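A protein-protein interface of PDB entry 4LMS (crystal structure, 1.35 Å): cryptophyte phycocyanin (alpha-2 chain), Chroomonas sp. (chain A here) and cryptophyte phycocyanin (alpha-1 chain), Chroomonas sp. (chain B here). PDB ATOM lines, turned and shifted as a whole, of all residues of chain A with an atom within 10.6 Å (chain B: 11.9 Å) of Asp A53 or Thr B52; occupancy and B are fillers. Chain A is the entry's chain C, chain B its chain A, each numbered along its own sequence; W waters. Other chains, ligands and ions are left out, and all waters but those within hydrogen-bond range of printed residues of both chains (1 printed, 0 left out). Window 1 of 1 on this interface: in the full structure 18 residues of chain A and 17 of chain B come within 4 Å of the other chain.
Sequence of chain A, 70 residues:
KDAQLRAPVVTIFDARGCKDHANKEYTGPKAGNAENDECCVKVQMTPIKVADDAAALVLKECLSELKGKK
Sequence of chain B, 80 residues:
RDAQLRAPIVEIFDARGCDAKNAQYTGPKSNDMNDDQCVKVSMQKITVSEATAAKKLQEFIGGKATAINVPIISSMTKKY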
ATOM      1  N   ILE A  48      -3.663 -36.147  33.681  1.00  0.00           N
ATOM      2  CA  ILE A  48      -4.582 -35.509  32.760  1.00  0.00           C
ATOM      3  C   ILE A  48      -4.715 -34.037  33.140  1.00  0.00           C
ATOM      4  O   ILE A  48      -5.028 -33.703  34.286  1.00  0.00           O
ATOM      5  CB  ILE A  48      -5.964 -36.199  32.750  1.00  0.00           C
ATOM      6  CG1 ILE A  48      -5.814 -37.693  32.478  1.00  0.00           C
ATOM      7  CG2 ILE A  48      -6.861 -35.504  31.710  1.00  0.00           C
ATOM      8  CD1 ILE A  48      -5.076 -38.023  31.205  1.00  0.00           C
ATOM      9  N   LYS A  49      -4.472 -33.166  32.167  1.00  0.00           N
ATOM     10  CA  LYS A  49      -4.495 -31.711  32.376  1.00  0.00           C
ATOM     11  C   LYS A  49      -5.326 -31.085  31.276  1.00  0.00           C
ATOM     12  O   LYS A  49      -5.378 -31.620  30.175  1.00  0.00           O
ATOM     13  CB  LYS A  49      -3.079 -31.126  32.281  1.00  0.00           C
ATOM     14  CG  LYS A  49      -2.053 -31.766  33.176  1.00  0.00           C
ATOM     15  CD  LYS A  49      -2.212 -31.329  34.592  1.00  0.00           C
ATOM     16  CE  LYS A  49      -1.060 -31.829  35.431  1.00  0.00           C
ATOM     17  NZ  LYS A  49      -1.212 -31.361  36.822  1.00  0.00           N
ATOM     18  N   VAL A  50      -5.971 -29.979  31.596  1.00  0.00           N
ATOM     19  CA  VAL A  50      -6.652 -29.142  30.595  1.00  0.00           C
ATOM     20  C   VAL A  50      -6.152 -27.724  30.780  1.00  0.00           C
ATOM     21  O   VAL A  50      -6.255 -27.182  31.880  1.00  0.00           O
ATOM     22  CB  VAL A  50      -8.178 -29.177  30.770  1.00  0.00           C
ATOM     23  CG1 VAL A  50      -8.853 -28.210  29.811  1.00  0.00           C
ATOM     24  CG2 VAL A  50      -8.712 -30.579  30.534  1.00  0.00           C
ATOM     25  N   ALA A  51      -5.598 -27.148  29.716  1.00  0.00           N
ATOM     26  CA  ALA A  51      -5.042 -25.792  29.761  1.00  0.00           C
ATOM     27  C   ALA A  51      -6.127 -24.736  29.622  1.00  0.00           C
ATOM     28  O   ALA A  51      -7.221 -24.978  29.122  1.00  0.00           O
ATOM     29  CB  ALA A  51      -4.026 -25.615  28.665  1.00  0.00           C
ATOM     30  N   ASP A  52      -5.794 -23.533  30.075  1.00  0.00           N
ATOM     31  CA  ASP A  52      -6.679 -22.387  30.039  1.00  0.00           C
ATOM     32  C   ASP A  52      -7.267 -22.146  28.661  1.00  0.00           C
ATOM     33  O   ASP A  52      -8.449 -21.811  28.543  1.00  0.00           O
ATOM     34  CB  ASP A  52      -5.860 -21.147  30.477  1.00  0.00           C
ATOM     35  CG  ASP A  52      -6.663 -19.834  30.480  1.00  0.00           C
ATOM     36  OD1 ASP A  52      -7.022 -19.346  31.587  1.00  0.00           O
ATOM     37  OD2 ASP A  52      -6.883 -19.244  29.389  1.00  0.00           O
ATOM     38  N   ASP A  53      -6.451 -22.261  27.617  1.00  0.00           N
ATOM     39  CA  ASP A  53      -6.949 -21.972  26.263  1.00  0.00           C
ATOM     40  C   ASP A  53      -8.052 -22.943  25.877  1.00  0.00           C
ATOM     41  O   ASP A  53      -9.036 -22.543  25.278  1.00  0.00           O
ATOM     42  CB  ASP A  53      -5.823 -21.990  25.208  1.00  0.00           C
ATOM     43  CG  ASP A  53      -5.059 -23.324  25.170  1.00  0.00           C
ATOM     44  OD1 ASP A  53      -4.487 -23.723  26.208  1.00  0.00           O
ATOM     45  OD2 ASP A  53      -5.036 -23.985  24.108  1.00  0.00           O
ATOM     46  N   ALA A  54      -7.902 -24.220  26.236  1.00  0.00           N
ATOM     47  CA  ALA A  54      -8.903 -25.202  25.844  1.00  0.00           C
ATOM     48  C   ALA A  54     -10.215 -24.924  26.571  1.00  0.00           C
ATOM     49  O   ALA A  54     -11.282 -24.955  25.959  1.00  0.00           O
ATOM     50  CB  ALA A  54      -8.381 -26.611  26.123  1.00  0.00           C
ATOM     51  N   ALA A  55     -10.141 -24.629  27.865  1.00  0.00           N
ATOM     52  CA  ALA A  55     -11.332 -24.333  28.653  1.00  0.00           C
ATOM     53  C   ALA A  55     -12.016 -23.050  28.180  1.00  0.00           C
ATOM     54  O   ALA A  55     -13.242 -22.959  28.137  1.00  0.00           O
ATOM     55  CB  ALA A  55     -10.987 -24.219  30.147  1.00  0.00           C
ATOM     56  N   ALA A  56     -11.216 -22.063  27.813  1.00  0.00           N
ATOM     57  CA  ALA A  56     -11.772 -20.790  27.371  1.00  0.00           C
ATOM     58  C   ALA A  56     -12.551 -20.953  26.063  1.00  0.00           C
ATOM     59  O   ALA A  56     -13.620 -20.348  25.861  1.00  0.00           O
ATOM     60  CB  ALA A  56     -10.671 -19.739  27.220  1.00  0.00           C
ATOM     61  N   LEU A  57     -12.038 -21.800  25.179  1.00  0.00           N
ATOM     62  CA  LEU A  57     -12.702 -22.014  23.891  1.00  0.00           C
ATOM     63  C   LEU A  57     -14.029 -22.786  24.075  1.00  0.00           C
ATOM     64  O   LEU A  57     -15.027 -22.450  23.456  1.00  0.00           O
ATOM     65  CB  LEU A  57     -11.753 -22.707  22.921  1.00  0.00           C
ATOM     66  CG  LEU A  57     -12.287 -22.983  21.516  1.00  0.00           C
ATOM     67  CD1 LEU A  57     -12.789 -21.726  20.858  1.00  0.00           C
ATOM     68  CD2 LEU A  57     -11.203 -23.608  20.648  1.00  0.00           C
ATOM     69  N   VAL A  58     -14.049 -23.775  24.966  1.00  0.00           N
ATOM     70  CA  VAL A  58     -15.293 -24.459  25.270  1.00  0.00           C
ATOM     71  C   VAL A  58     -16.328 -23.477  25.828  1.00  0.00           C
ATOM     72  O   VAL A  58     -17.502 -23.530  25.482  1.00  0.00           O
ATOM     73  CB  VAL A  58     -15.081 -25.662  26.220  1.00  0.00           C
ATOM     74  CG1 VAL A  58     -16.416 -26.281  26.614  1.00  0.00           C
ATOM     75  CG2 VAL A  58     -14.183 -26.711  25.555  1.00  0.00           C
ATOM     76  N   LEU A  59     -15.908 -22.602  26.734  1.00  0.00           N
ATOM     77  CA  LEU A  59     -16.830 -21.610  27.285  1.00  0.00           C
ATOM     78  C   LEU A  59     -17.411 -20.710  26.181  1.00  0.00           C
ATOM     79  O   LEU A  59     -18.617 -20.445  26.165  1.00  0.00           O
ATOM     80  CB  LEU A  59     -16.121 -20.760  28.334  1.00  0.00           C
ATOM     81  CG  LEU A  59     -16.965 -19.627  28.922  1.00  0.00           C
ATOM     82  CD1 LEU A  59     -18.164 -20.158  29.652  1.00  0.00           C
ATOM     83  CD2 LEU A  59     -16.139 -18.745  29.815  1.00  0.00           C
ATOM     84  N   LYS A  60     -16.579 -20.259  25.245  1.00  0.00           N
ATOM     85  CA  LYS A  60     -17.101 -19.498  24.112  1.00  0.00           C
ATOM     86  C   LYS A  60     -18.181 -20.280  23.355  1.00  0.00           C
ATOM     87  O   LYS A  60     -19.218 -19.715  22.979  1.00  0.00           O
ATOM     88  CB  LYS A  60     -15.981 -19.094  23.151  1.00  0.00           C
ATOM     89  CG  LYS A  60     -15.044 -18.020  23.697  1.00  0.00           C
ATOM     90  CD  LYS A  60     -14.066 -17.518  22.647  1.00  0.00           C
ATOM     91  CE  LYS A  60     -13.156 -16.406  23.197  1.00  0.00           C
ATOM     92  NZ  LYS A  60     -12.238 -16.874  24.309  1.00  0.00           N
ATOM     93  N   GLU A  61     -17.953 -21.574  23.100  1.00  0.00           N
ATOM     94  CA  GLU A  61     -18.989 -22.364  22.426  1.00  0.00           C
ATOM     95  C   GLU A  61     -20.275 -22.365  23.260  1.00  0.00           C
ATOM     96  O   GLU A  61     -21.374 -22.175  22.731  1.00  0.00           O
ATOM     97  CB  GLU A  61     -18.550 -23.798  22.185  1.00  0.00           C
ATOM     98  CG  GLU A  61     -17.385 -23.976  21.245  1.00  0.00           C
ATOM     99  CD  GLU A  61     -17.044 -25.463  21.042  1.00  0.00           C
ATOM    100  OE1 GLU A  61     -17.710 -26.348  21.643  1.00  0.00           O
ATOM    101  OE2 GLU A  61     -16.102 -25.731  20.271  1.00  0.00           O
ATOM    102  N   ILE B   9     -13.969 -12.538  17.559  1.00  0.00           N
ATOM    103  CA  ILE B   9     -14.759 -13.506  18.310  1.00  0.00           C
ATOM    104  C   ILE B   9     -16.206 -13.041  18.245  1.00  0.00           C
ATOM    105  O   ILE B   9     -16.560 -12.005  18.822  1.00  0.00           O
ATOM    106  CB  ILE B   9     -14.344 -13.568  19.795  1.00  0.00           C
ATOM    107  CG1 ILE B   9     -12.842 -13.792  19.931  1.00  0.00           C
ATOM    108  CG2 ILE B   9     -15.130 -14.645  20.536  1.00  0.00           C
ATOM    109  CD1 ILE B   9     -12.346 -14.940  19.156  1.00  0.00           C
ATOM    110  N   GLN B  44      -9.815 -10.487  19.620  1.00  0.00           N
ATOM    111  CA  GLN B  44      -8.989 -11.106  20.647  1.00  0.00           C
ATOM    112  C   GLN B  44      -7.836 -11.850  20.017  1.00  0.00           C
ATOM    113  O   GLN B  44      -7.985 -12.439  18.942  1.00  0.00           O
ATOM    114  CB  GLN B  44      -9.832 -12.093  21.469  1.00  0.00           C
ATOM    115  CG  GLN B  44     -10.887 -11.430  22.343  1.00  0.00           C
ATOM    116  CD  GLN B  44     -11.601 -12.414  23.253  1.00  0.00           C
ATOM    117  OE1 GLN B  44     -11.042 -13.449  23.642  1.00  0.00           O
ATOM    118  NE2 GLN B  44     -12.846 -12.095  23.602  1.00  0.00           N
ATOM    119  N   LYS B  45      -6.697 -11.840  20.701  1.00  0.00           N
ATOM    120  CA  LYS B  45      -5.550 -12.645  20.301  1.00  0.00           C
ATOM    121  C   LYS B  45      -5.951 -14.103  20.325  1.00  0.00           C
ATOM    122  O   LYS B  45      -6.559 -14.560  21.288  1.00  0.00           O
ATOM    123  CB  LYS B  45      -4.373 -12.434  21.253  1.00  0.00           C
ATOM    124  CG  LYS B  45      -3.842 -10.993  21.250  1.00  0.00           C
ATOM    125  CD  LYS B  45      -2.695 -10.781  22.246  1.00  0.00           C
ATOM    126  CE  LYS B  45      -3.154 -11.022  23.685  1.00  0.00           C
ATOM    127  NZ  LYS B  45      -2.085 -10.766  24.696  1.00  0.00           N
ATOM    128  N   ILE B  46      -5.590 -14.830  19.278  1.00  0.00           N
ATOM    129  CA  ILE B  46      -5.905 -16.251  19.218  1.00  0.00           C
ATOM    130  C   ILE B  46      -4.647 -17.016  19.583  1.00  0.00           C
ATOM    131  O   ILE B  46      -3.589 -16.794  19.008  1.00  0.00           O
ATOM    132  CB  ILE B  46      -6.390 -16.679  17.830  1.00  0.00           C
ATOM    133  CG1 ILE B  46      -7.583 -15.811  17.398  1.00  0.00           C
ATOM    134  CG2 ILE B  46      -6.702 -18.202  17.835  1.00  0.00           C
ATOM    135  CD1 ILE B  46      -8.705 -15.742  18.415  1.00  0.00           C
ATOM    136  N   THR B  47      -4.767 -17.922  20.548  1.00  0.00           N
ATOM    137  CA  THR B  47      -3.621 -18.675  21.023  1.00  0.00           C
ATOM    138  C   THR B  47      -4.018 -20.130  21.279  1.00  0.00           C
ATOM    139  O   THR B  47      -5.171 -20.440  21.638  1.00  0.00           O
ATOM    140  CB  THR B  47      -3.040 -18.071  22.301  1.00  0.00           C
ATOM    141  OG1 THR B  47      -1.816 -18.742  22.639  1.00  0.00           O
ATOM    142  CG2 THR B  47      -4.019 -18.172  23.447  1.00  0.00           C
ATOM    143  N   VAL B  48      -3.041 -21.008  21.063  1.00  0.00           N
ATOM    144  CA  VAL B  48      -3.162 -22.421  21.367  1.00  0.00           C
ATOM    145  C   VAL B  48      -1.875 -22.804  22.074  1.00  0.00           C
ATOM    146  O   VAL B  48      -0.789 -22.488  21.597  1.00  0.00           O
ATOM    147  CB  VAL B  48      -3.322 -23.279  20.109  1.00  0.00           C
ATOM    148  CG1 VAL B  48      -3.345 -24.761  20.483  1.00  0.00           C
ATOM    149  CG2 VAL B  48      -4.608 -22.906  19.373  1.00  0.00           C
ATOM    150  N   SER B  49      -1.999 -23.416  23.234  1.00  0.00           N
ATOM    151  CA  SER B  49      -0.832 -23.754  24.032  1.00  0.00           C
ATOM    152  C   SER B  49      -0.166 -25.011  23.486  1.00  0.00           C
ATOM    153  O   SER B  49      -0.810 -25.837  22.843  1.00  0.00           O
ATOM    154  CB  SER B  49      -1.249 -23.971  25.482  1.00  0.00           C
ATOM    155  OG  SER B  49      -2.087 -25.118  25.596  1.00  0.00           O
ATOM    156  N   GLU B  50       1.125 -25.164  23.745  1.00  0.00           N
ATOM    157  CA  GLU B  50       1.820 -26.361  23.312  1.00  0.00           C
ATOM    158  C   GLU B  50       1.270 -27.595  24.040  1.00  0.00           C
ATOM    159  O   GLU B  50       1.259 -28.676  23.469  1.00  0.00           O
ATOM    160  CB  GLU B  50       3.341 -26.211  23.513  1.00  0.00           C
ATOM    161  CG  GLU B  50       3.944 -25.202  22.529  1.00  0.00           C
ATOM    162  CD  GLU B  50       5.446 -25.195  22.571  1.00  0.00           C
ATOM    163  OE1 GLU B  50       5.996 -26.055  23.277  1.00  0.00           O
ATOM    164  OE2 GLU B  50       6.070 -24.332  21.919  1.00  0.00           O
ATOM    165  N   ALA B  51       0.802 -27.432  25.271  1.00  0.00           N
ATOM    166  CA  ALA B  51       0.139 -28.532  25.988  1.00  0.00           C
ATOM    167  C   ALA B  51      -1.115 -29.011  25.269  1.00  0.00           C
ATOM    168  O   ALA B  51      -1.322 -30.203  25.117  1.00  0.00           O
ATOM    169  CB  ALA B  51      -0.231 -28.116  27.391  1.00  0.00           C
ATOM    170  N   THR B  52      -1.977 -28.089  24.863  1.00  0.00           N
ATOM    171  CA  THR B  52      -3.113 -28.487  24.053  1.00  0.00           C
ATOM    172  C   THR B  52      -2.650 -29.156  22.761  1.00  0.00           C
ATOM    173  O   THR B  52      -3.196 -30.176  22.345  1.00  0.00           O
ATOM    174  CB  THR B  52      -3.999 -27.272  23.740  1.00  0.00           C
ATOM    175  OG1 THR B  52      -4.542 -26.786  24.967  1.00  0.00           O
ATOM    176  CG2 THR B  52      -5.137 -27.645  22.814  1.00  0.00           C
ATOM    177  N   ALA B  53      -1.654 -28.564  22.106  1.00  0.00           N
ATOM    178  CA  ALA B  53      -1.148 -29.119  20.855  1.00  0.00           C
ATOM    179  C   ALA B  53      -0.660 -30.556  21.032  1.00  0.00           C
ATOM    180  O   ALA B  53      -0.810 -31.395  20.138  1.00  0.00           O
ATOM    181  CB  ALA B  53      -0.036 -28.257  20.306  1.00  0.00           C
ATOM    182  N   ALA B  54      -0.020 -30.840  22.161  1.00  0.00           N
ATOM    183  CA  ALA B  54       0.462 -32.190  22.409  1.00  0.00           C
ATOM    184  C   ALA B  54      -0.710 -33.163  22.544  1.00  0.00           C
ATOM    185  O   ALA B  54      -0.654 -34.273  22.054  1.00  0.00           O
ATOM    186  CB  ALA B  54       1.341 -32.230  23.663  1.00  0.00           C
ATOM    187  N   LYS B  55      -1.786 -32.703  23.167  1.00  0.00           N
ATOM    188  CA  LYS B  55      -2.970 -33.538  23.292  1.00  0.00           C
ATOM    189  C   LYS B  55      -3.602 -33.793  21.927  1.00  0.00           C
ATOM    190  O   LYS B  55      -4.013 -34.913  21.636  1.00  0.00           O
ATOM    191  CB  LYS B  55      -3.989 -32.920  24.236  1.00  0.00           C
ATOM    192  CG  LYS B  55      -3.506 -32.815  25.671  1.00  0.00           C
ATOM    193  CD  LYS B  55      -4.538 -32.158  26.569  1.00  0.00           C
ATOM    194  CE  LYS B  55      -5.680 -33.106  26.885  1.00  0.00           C
ATOM    195  NZ  LYS B  55      -6.640 -32.515  27.848  1.00  0.00           N
ATOM    196  N   LYS B  56      -3.634 -32.769  21.076  1.00  0.00           N
ATOM    197  CA  LYS B  56      -4.185 -32.938  19.737  1.00  0.00           C
ATOM    198  C   LYS B  56      -3.337 -33.920  18.902  1.00  0.00           C
ATOM    199  O   LYS B  56      -3.873 -34.755  18.187  1.00  0.00           O
ATOM    200  CB  LYS B  56      -4.334 -31.587  19.026  1.00  0.00           C
ATOM    201  CG  LYS B  56      -5.250 -30.599  19.758  1.00  0.00           C
ATOM    202  CD  LYS B  56      -6.631 -31.177  20.038  1.00  0.00           C
ATOM    203  CE  LYS B  56      -7.377 -31.550  18.760  1.00  0.00           C
ATOM    204  NZ  LYS B  56      -8.770 -32.026  19.067  1.00  0.00           N
ATOM    205  N   LEU B  57      -2.011 -33.827  19.001  1.00  0.00           N
ATOM    206  CA  LEU B  57      -1.134 -34.746  18.272  1.00  0.00           C
ATOM    207  C   LEU B  57      -1.481 -36.190  18.638  1.00  0.00           C
ATOM    208  O   LEU B  57      -1.649 -37.043  17.767  1.00  0.00           O
ATOM    209  CB  LEU B  57       0.329 -34.466  18.603  1.00  0.00           C
ATOM    210  CG  LEU B  57       1.310 -35.510  18.062  1.00  0.00           C
ATOM    211  CD1 LEU B  57       1.320 -35.537  16.529  1.00  0.00           C
ATOM    212  CD2 LEU B  57       2.719 -35.297  18.618  1.00  0.00           C
ATOM    213  N   GLN B  58      -1.693 -36.460  19.917  1.00  0.00           N
ATOM    214  CA  GLN B  58      -2.016 -37.814  20.349  1.00  0.00           C
ATOM    215  C   GLN B  58      -3.340 -38.309  19.772  1.00  0.00           C
ATOM    216  O   GLN B  58      -3.490 -39.493  19.459  1.00  0.00           O
ATOM    217  CB  GLN B  58      -1.983 -37.914  21.872  1.00  0.00           C
ATOM    218  CG  GLN B  58      -2.155 -39.313  22.405  1.00  0.00           C
ATOM    219  CD  GLN B  58      -3.582 -39.759  22.506  1.00  0.00           C
ATOM    220  OE1 GLN B  58      -4.504 -38.959  22.668  1.00  0.00           O
ATOM    221  NE2 GLN B  58      -3.781 -41.058  22.403  1.00  0.00           N
ATOM    222  N   GLU B  59      -4.288 -37.383  19.599  1.00  0.00           N
ATOM    223  CA  GLU B  59      -5.544 -37.703  18.924  1.00  0.00           C
ATOM    224  C   GLU B  59      -5.400 -37.959  17.430  1.00  0.00           C
ATOM    225  O   GLU B  59      -6.153 -38.764  16.854  1.00  0.00           O
ATOM    226  CB  GLU B  59      -6.560 -36.594  19.145  1.00  0.00           C
ATOM    227  CG  GLU B  59      -6.958 -36.425  20.588  1.00  0.00           C
ATOM    228  CD  GLU B  59      -7.906 -35.284  20.812  1.00  0.00           C
ATOM    229  OE1 GLU B  59      -8.180 -34.516  19.870  1.00  0.00           O
ATOM    230  OE2 GLU B  59      -8.361 -35.129  21.951  1.00  0.00           O
ATOM    231  N   PHE B  60      -4.477 -37.242  16.795  1.00  0.00           N
ATOM    232  CA  PHE B  60      -4.323 -37.255  15.343  1.00  0.00           C
ATOM    233  C   PHE B  60      -3.392 -38.356  14.820  1.00  0.00           C
ATOM    234  O   PHE B  60      -3.444 -38.720  13.643  1.00  0.00           O
ATOM    235  CB  PHE B  60      -3.718 -35.934  14.858  1.00  0.00           C
ATOM    236  CG  PHE B  60      -4.534 -34.708  15.163  1.00  0.00           C
ATOM    237  CD1 PHE B  60      -5.872 -34.771  15.547  1.00  0.00           C
ATOM    238  CD2 PHE B  60      -3.951 -33.458  15.014  1.00  0.00           C
ATOM    239  CE1 PHE B  60      -6.588 -33.603  15.783  1.00  0.00           C
ATOM    240  CE2 PHE B  60      -4.652 -32.320  15.262  1.00  0.00           C
ATOM    241  CZ  PHE B  60      -5.972 -32.386  15.650  1.00  0.00           C
ATOM    242  N   ILE B  61      -2.509 -38.850  15.677  1.00  0.00           N
ATOM    243  CA  ILE B  61      -1.368 -39.645  15.236  1.00  0.00           C
ATOM    244  C   ILE B  61      -1.734 -41.059  14.763  1.00  0.00           C
ATOM    245  O   ILE B  61      -1.018 -41.642  13.940  1.00  0.00           O
ATOM    246  CB  ILE B  61      -0.267 -39.637  16.329  1.00  0.00           C
ATOM    247  CG1 ILE B  61       1.087 -40.076  15.779  1.00  0.00           C
ATOM    248  CG2 ILE B  61      -0.665 -40.497  17.503  1.00  0.00           C
ATOM    249  CD1 ILE B  61       2.212 -39.817  16.764  1.00  0.00           C
HETATM  250  O   HOH W   1      -5.379 -28.477  27.128  1.00  0.00           O
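Printed residues of chain B within 4 Å of Lys A49: Lys B55.
Of the printed residues of chain B, Val A50 touches Lys B55 (3.9 Å).
Of chain B, only Ser B49 and Thr B52 come within 4 Å of Ala A51.
No residue of chain B comes within 4 Å of Asp A52.
Asp A53 touches just these residues of chain B: Thr B47 (3.9 Å), Val B48 (3.7 Å), Ser B49 (2.8 Å) and Thr B52 (3.0 Å).
No residue of chain B comes within 4 Å of Ala A55.
Ala A56 touches none of the printed residues of chain B.
No residue of chain B comes within 4 Å of Leu A57.
Glu A61 touches none of the printed residues of chain B.
Of the printed residues of chain A, Ile B9 touches Lys A60.
Of the printed residues of chain A, Gln B44 touches Lys A60 (3.7 Å).
Thr B47 touches one residue of chain A.
Of chain A, only Ala A51 (3.7 Å) and Asp A53 (2.8 Å) come within 4 Å of Ser B49.
No residue of chain A comes within 4 Å of Ala B51.
No residue of chain A comes within 4 Å of Ala B53.
No residue of chain A comes within 4 Å of Ala B54.
Lys B56 touches none of the printed residues of chain A.
The nearest printed residue of chain A that does not touch Thr B52 is Ala A54 (4.01 Å).
Water W1 bridges OG1 of Thr B52 (2.9 Å) and N of Ala A51 (2.9 Å).
NZ of Lys B55 lies within hydrogen-bond range of O of Lys A49.
The side-chain hydroxyl (OG1) of Thr B52 is in hydrogen-bond range of the side-chain carboxylate (OD2) of Asp A53, at 3.0 Å.
OG of Ser B49 is in hydrogen-bond range of OD1 of Asp A53.
NZ of Lys B55 touches CG2 of Val A50 (3.9 Å).
CB of Ala A51 touches OG of Ser B49, 3.7 Å away.
CB of Ala A51 touches OG1 of Thr B52, 3.9 Å away.
O of Thr B47 touches CB of Asp A53 (3.9 Å).
Asp A53 touches Val B48 (OD2 to CA, 3.7 Å).
CD of Lys A60 touches CG2 of Ile B9, 3.7 Å away.
Lys A60 touches Gln B44.
The side-chain hydroxyl (OG) of Ser B49 is in hydrogen-bond range of the side-chain hydroxyl (OG1) of Thr B52.
Printed residues of chain B that touch a printed residue of chain A: Ile B9, Gln B44, Thr B47, Val B48, Ser B49, Thr B52 and Lys B55.
Of the 14 printed residues of chain A, 5 touch a printed residue of chain B.
Hydrophobic or aromatic side chains of chain A that line the printed part of chain B: Val A50 and Ala A51.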
